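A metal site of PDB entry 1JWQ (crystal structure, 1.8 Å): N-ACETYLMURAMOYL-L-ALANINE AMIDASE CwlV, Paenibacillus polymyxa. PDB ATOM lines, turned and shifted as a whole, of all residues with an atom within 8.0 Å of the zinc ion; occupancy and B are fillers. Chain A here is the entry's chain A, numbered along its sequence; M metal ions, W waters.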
ATOM      1  N   ALA A   8      -9.820   6.304 -21.395  1.00  0.00           N
ATOM      2  CA  ALA A   8     -10.793   5.875 -22.399  1.00  0.00           C
ATOM      3  C   ALA A   8     -11.727   4.931 -21.644  1.00  0.00           C
ATOM      4  O   ALA A   8     -11.323   3.838 -21.267  1.00  0.00           O
ATOM      5  CB  ALA A   8     -10.101   5.135 -23.535  1.00  0.00           C
ATOM      6  N   GLY A   9     -12.967   5.355 -21.446  1.00  0.00           N
ATOM      7  CA  GLY A   9     -13.911   4.552 -20.716  1.00  0.00           C
ATOM      8  C   GLY A   9     -14.119   3.142 -21.234  1.00  0.00           C
ATOM      9  O   GLY A   9     -14.039   2.879 -22.441  1.00  0.00           O
ATOM     10  N   HIS A  10     -14.376   2.223 -20.301  1.00  0.00           N
ATOM     11  CA  HIS A  10     -14.650   0.832 -20.611  1.00  0.00           C
ATOM     12  C   HIS A  10     -13.480   0.098 -21.255  1.00  0.00           C
ATOM     13  O   HIS A  10     -12.330   0.513 -21.130  1.00  0.00           O
ATOM     14  CB  HIS A  10     -15.882   0.785 -21.517  1.00  0.00           C
ATOM     15  CG  HIS A  10     -16.989   1.669 -21.034  1.00  0.00           C
ATOM     16  ND1 HIS A  10     -17.670   1.441 -19.860  1.00  0.00           N
ATOM     17  CD2 HIS A  10     -17.446   2.854 -21.511  1.00  0.00           C
ATOM     18  CE1 HIS A  10     -18.502   2.438 -19.632  1.00  0.00           C
ATOM     19  NE2 HIS A  10     -18.386   3.317 -20.616  1.00  0.00           N
ATOM     20  N   ASP A  14     -15.987  -5.014 -21.227  1.00  0.00           N
ATOM     21  CA  ASP A  14     -16.914  -3.894 -21.032  1.00  0.00           C
ATOM     22  C   ASP A  14     -16.932  -3.071 -22.320  1.00  0.00           C
ATOM     23  O   ASP A  14     -16.033  -2.283 -22.584  1.00  0.00           O
ATOM     24  CB  ASP A  14     -16.454  -3.009 -19.861  1.00  0.00           C
ATOM     25  CG  ASP A  14     -17.428  -1.877 -19.567  1.00  0.00           C
ATOM     26  OD1 ASP A  14     -18.539  -1.868 -20.150  1.00  0.00           O
ATOM     27  OD2 ASP A  14     -17.090  -1.002 -18.740  1.00  0.00           O
ATOM     28  N   SER A  15     -17.961  -3.278 -23.129  1.00  0.00           N
ATOM     29  CA  SER A  15     -18.083  -2.574 -24.393  1.00  0.00           C
ATOM     30  C   SER A  15     -18.655  -1.166 -24.215  1.00  0.00           C
ATOM     31  O   SER A  15     -18.557  -0.342 -25.124  1.00  0.00           O
ATOM     32  CB  SER A  15     -18.985  -3.344 -25.344  1.00  0.00           C
ATOM     33  OG  SER A  15     -20.300  -3.419 -24.818  1.00  0.00           O
ATOM     34  N   GLY A  16     -19.224  -0.904 -23.049  1.00  0.00           N
ATOM     35  CA  GLY A  16     -19.842   0.388 -22.830  1.00  0.00           C
ATOM     36  C   GLY A  16     -21.148   0.338 -23.613  1.00  0.00           C
ATOM     37  O   GLY A  16     -21.673  -0.752 -23.846  1.00  0.00           O
ATOM     38  N   ALA A  17     -21.660   1.487 -24.027  1.00  0.00           N
ATOM     39  CA  ALA A  17     -22.904   1.527 -24.784  1.00  0.00           C
ATOM     40  C   ALA A  17     -22.731   0.949 -26.184  1.00  0.00           C
ATOM     41  O   ALA A  17     -21.688   1.092 -26.808  1.00  0.00           O
ATOM     42  CB  ALA A  17     -23.419   2.957 -24.865  1.00  0.00           C
ATOM     43  N   GLU A  26     -19.073   1.683 -27.622  1.00  0.00           N
ATOM     44  CA  GLU A  26     -18.541   2.906 -27.018  1.00  0.00           C
ATOM     45  C   GLU A  26     -17.046   2.776 -26.705  1.00  0.00           C
ATOM     46  O   GLU A  26     -16.282   3.720 -26.898  1.00  0.00           O
ATOM     47  CB  GLU A  26     -19.300   3.228 -25.737  1.00  0.00           C
ATOM     48  CG  GLU A  26     -18.743   4.436 -24.987  1.00  0.00           C
ATOM     49  CD  GLU A  26     -19.289   4.548 -23.581  1.00  0.00           C
ATOM     50  OE1 GLU A  26     -18.753   5.373 -22.807  1.00  0.00           O
ATOM     51  OE2 GLU A  26     -20.244   3.814 -23.252  1.00  0.00           O
ATOM     52  N   LYS A  27     -16.631   1.606 -26.234  1.00  0.00           N
ATOM     53  CA  LYS A  27     -15.225   1.399 -25.888  1.00  0.00           C
ATOM     54  C   LYS A  27     -14.298   1.703 -27.052  1.00  0.00           C
ATOM     55  O   LYS A  27     -13.184   2.201 -26.870  1.00  0.00           O
ATOM     56  CB  LYS A  27     -14.983  -0.047 -25.399  1.00  0.00           C
ATOM     57  CG  LYS A  27     -15.210  -1.122 -26.459  1.00  0.00           C
ATOM     58  CD  LYS A  27     -14.701  -2.474 -25.973  1.00  0.00           C
ATOM     59  CE  LYS A  27     -14.823  -3.545 -27.059  1.00  0.00           C
ATOM     60  NZ  LYS A  27     -14.182  -4.840 -26.652  1.00  0.00           N
ATOM     61  N   ASN A  30     -14.147   5.535 -27.415  1.00  0.00           N
ATOM     62  CA  ASN A  30     -13.351   6.094 -26.337  1.00  0.00           C
ATOM     63  C   ASN A  30     -11.855   5.938 -26.561  1.00  0.00           C
ATOM     64  O   ASN A  30     -11.087   6.876 -26.343  1.00  0.00           O
ATOM     65  CB  ASN A  30     -13.738   5.469 -24.994  1.00  0.00           C
ATOM     66  CG  ASN A  30     -15.183   5.751 -24.609  1.00  0.00           C
ATOM     67  OD1 ASN A  30     -15.785   6.697 -25.112  1.00  0.00           O
ATOM     68  ND2 ASN A  30     -15.726   4.948 -23.697  1.00  0.00           N
ATOM     69  N   SER A  78     -11.729  11.669 -18.557  1.00  0.00           N
ATOM     70  CA  SER A  78     -12.283  10.384 -18.934  1.00  0.00           C
ATOM     71  C   SER A  78     -13.167  10.656 -20.151  1.00  0.00           C
ATOM     72  O   SER A  78     -14.003  11.552 -20.128  1.00  0.00           O
ATOM     73  CB  SER A  78     -13.099   9.782 -17.791  1.00  0.00           C
ATOM     74  OG  SER A  78     -13.474   8.453 -18.110  1.00  0.00           O
ATOM     75  N   ILE A  79     -12.962   9.884 -21.214  1.00  0.00           N
ATOM     76  CA  ILE A  79     -13.717  10.050 -22.447  1.00  0.00           C
ATOM     77  C   ILE A  79     -14.735   8.938 -22.627  1.00  0.00           C
ATOM     78  O   ILE A  79     -14.416   7.754 -22.552  1.00  0.00           O
ATOM     79  CB  ILE A  79     -12.773  10.094 -23.663  1.00  0.00           C
ATOM     80  CG1 ILE A  79     -11.784  11.259 -23.517  1.00  0.00           C
ATOM     81  CG2 ILE A  79     -13.586  10.271 -24.936  1.00  0.00           C
ATOM     82  CD1 ILE A  79     -10.761  11.359 -24.647  1.00  0.00           C
ATOM     83  N   HIS A  80     -15.979   9.352 -22.850  1.00  0.00           N
ATOM     84  CA  HIS A  80     -17.092   8.426 -23.010  1.00  0.00           C
ATOM     85  C   HIS A  80     -18.047   8.853 -24.118  1.00  0.00           C
ATOM     86  O   HIS A  80     -17.925   9.943 -24.687  1.00  0.00           O
ATOM     87  CB  HIS A  80     -17.886   8.364 -21.703  1.00  0.00           C
ATOM     88  CG  HIS A  80     -17.159   7.666 -20.588  1.00  0.00           C
ATOM     89  ND1 HIS A  80     -17.474   6.388 -20.194  1.00  0.00           N
ATOM     90  CD2 HIS A  80     -16.155   8.081 -19.781  1.00  0.00           C
ATOM     91  CE1 HIS A  80     -16.685   6.033 -19.194  1.00  0.00           C
ATOM     92  NE2 HIS A  80     -15.875   7.043 -18.919  1.00  0.00           N
ATOM     93  N   ALA A  81     -18.988   7.978 -24.425  1.00  0.00           N
ATOM     94  CA  ALA A  81     -20.036   8.234 -25.416  1.00  0.00           C
ATOM     95  C   ALA A  81     -21.298   7.863 -24.638  1.00  0.00           C
ATOM     96  O   ALA A  81     -21.304   6.893 -23.874  1.00  0.00           O
ATOM     97  CB  ALA A  81     -19.868   7.345 -26.636  1.00  0.00           C
ATOM     98  N   ASN A  82     -22.363   8.636 -24.842  1.00  0.00           N
ATOM     99  CA  ASN A  82     -23.615   8.466 -24.112  1.00  0.00           C
ATOM    100  C   ASN A  82     -24.641   7.536 -24.766  1.00  0.00           C
ATOM    101  O   ASN A  82     -24.494   7.128 -25.920  1.00  0.00           O
ATOM    102  CB  ASN A  82     -24.228   9.850 -23.913  1.00  0.00           C
ATOM    103  CG  ASN A  82     -24.805  10.042 -22.526  1.00  0.00           C
ATOM    104  OD1 ASN A  82     -24.926  11.182 -22.061  1.00  0.00           O
ATOM    105  ND2 ASN A  82     -25.173   8.960 -21.870  1.00  0.00           N
ATOM    106  N   SER A  83     -25.678   7.216 -24.015  1.00  0.00           N
ATOM    107  CA  SER A  83     -26.751   6.362 -24.502  1.00  0.00           C
ATOM    108  C   SER A  83     -28.018   6.692 -23.737  1.00  0.00           C
ATOM    109  O   SER A  83     -27.978   6.984 -22.541  1.00  0.00           O
ATOM    110  CB  SER A  83     -26.409   4.885 -24.319  1.00  0.00           C
ATOM    111  OG  SER A  83     -27.333   4.081 -25.011  1.00  0.00           O
ATOM    112  N   LEU A 140     -15.358  14.156 -16.842  1.00  0.00           N
ATOM    113  CA  LEU A 140     -15.756  13.030 -17.672  1.00  0.00           C
ATOM    114  C   LEU A 140     -16.559  13.629 -18.817  1.00  0.00           C
ATOM    115  O   LEU A 140     -17.508  14.381 -18.604  1.00  0.00           O
ATOM    116  CB  LEU A 140     -16.596  12.029 -16.880  1.00  0.00           C
ATOM    117  CG  LEU A 140     -16.946  10.746 -17.639  1.00  0.00           C
ATOM    118  CD1 LEU A 140     -17.043   9.580 -16.658  1.00  0.00           C
ATOM    119  CD2 LEU A 140     -18.263  10.941 -18.386  1.00  0.00           C
ATOM    120  N   LEU A 141     -16.153  13.315 -20.033  1.00  0.00           N
ATOM    121  CA  LEU A 141     -16.815  13.849 -21.204  1.00  0.00           C
ATOM    122  C   LEU A 141     -17.684  12.805 -21.880  1.00  0.00           C
ATOM    123  O   LEU A 141     -17.233  11.697 -22.158  1.00  0.00           O
ATOM    124  CB  LEU A 141     -15.773  14.358 -22.204  1.00  0.00           C
ATOM    125  CG  LEU A 141     -14.649  15.233 -21.634  1.00  0.00           C
ATOM    126  CD1 LEU A 141     -13.687  15.610 -22.765  1.00  0.00           C
ATOM    127  CD2 LEU A 141     -15.235  16.487 -20.990  1.00  0.00           C
ATOM    128  N   GLU A 142     -18.941  13.160 -22.121  1.00  0.00           N
ATOM    129  CA  GLU A 142     -19.864  12.279 -22.841  1.00  0.00           C
ATOM    130  C   GLU A 142     -19.967  13.033 -24.150  1.00  0.00           C
ATOM    131  O   GLU A 142     -20.744  13.985 -24.285  1.00  0.00           O
ATOM    132  CB  GLU A 142     -21.210  12.208 -22.124  1.00  0.00           C
ATOM    133  CG  GLU A 142     -21.191  11.334 -20.865  1.00  0.00           C
ATOM    134  CD  GLU A 142     -21.032   9.848 -21.170  1.00  0.00           C
ATOM    135  OE1 GLU A 142     -20.881   9.053 -20.229  1.00  0.00           O
ATOM    136  OE2 GLU A 142     -21.070   9.490 -22.371  1.00  0.00           O
ATOM    137  N   LEU A 146     -24.713   7.518 -28.724  1.00  0.00           N
ATOM    138  CA  LEU A 146     -24.590   6.408 -29.662  1.00  0.00           C
ATOM    139  C   LEU A 146     -25.959   5.791 -29.919  1.00  0.00           C
ATOM    140  O   LEU A 146     -26.107   4.929 -30.786  1.00  0.00           O
ATOM    141  CB  LEU A 146     -23.659   5.344 -29.091  1.00  0.00           C
ATOM    142  CG  LEU A 146     -22.225   5.800 -28.855  1.00  0.00           C
ATOM    143  CD1 LEU A 146     -21.391   4.650 -28.297  1.00  0.00           C
ATOM    144  CD2 LEU A 146     -21.630   6.296 -30.174  1.00  0.00           C
HETATM  145 ZN    ZN M   1     -19.217   5.242 -20.817  1.00  0.00          ZN
HETATM  146  O   HOH W   1     -20.827   6.438 -21.018  1.00  0.00           O
HETATM  147  O   HOH W   2     -21.825   3.684 -20.969  1.00  0.00           O
HETATM  148  O   HOH W   3     -19.982   5.144 -18.707  1.00  0.00           O
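Within 4 Å of the zinc ion: His 10, Glu 26 and His 80.
The backbone carbonyl oxygen of Glu 26 sits close to the side-chain amide nitrogen of Asn 30. The side-chain carboxylate (OD2) of Asp 14 sits at hydrogen-bond distance from a ring nitrogen (ND1) of His 10 (2.7 Å). NE2 of His 80 lies within hydrogen-bond range of OG of Ser 78 (2.9 Å). The backbone NH of Glu 26 lies within hydrogen-bond range of the backbone carbonyl oxygen of Ala 17 (2.8 Å). The backbone NH (N) of Ala 81 lies close to the side-chain carboxylate (OE1) of Glu 26. The backbone NH (N) of His 80 sits at hydrogen-bond distance from the backbone carbonyl oxygen (O) of Leu 141, at 2.7 Å. N of His 80 sits close to OD1 of Asn 30, 3.5 Å away. The backbone NH (N) of Glu 26 is in hydrogen-bond range of the backbone carbonyl oxygen (O) of Ser 15 (3.3 Å).
The zinc ion is bound by water W1, at 2.0 Å. The side-chain carboxylate (OE1) of Glu 26 is bound to the zinc ion. NE2 of His 10 is bound to the zinc ion. A ring nitrogen (ND1) of His 80 is bound to the zinc ion. Water W3 binds the zinc ion, at 2.2 Å. The zinc ion has five donor atoms within binding distance.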
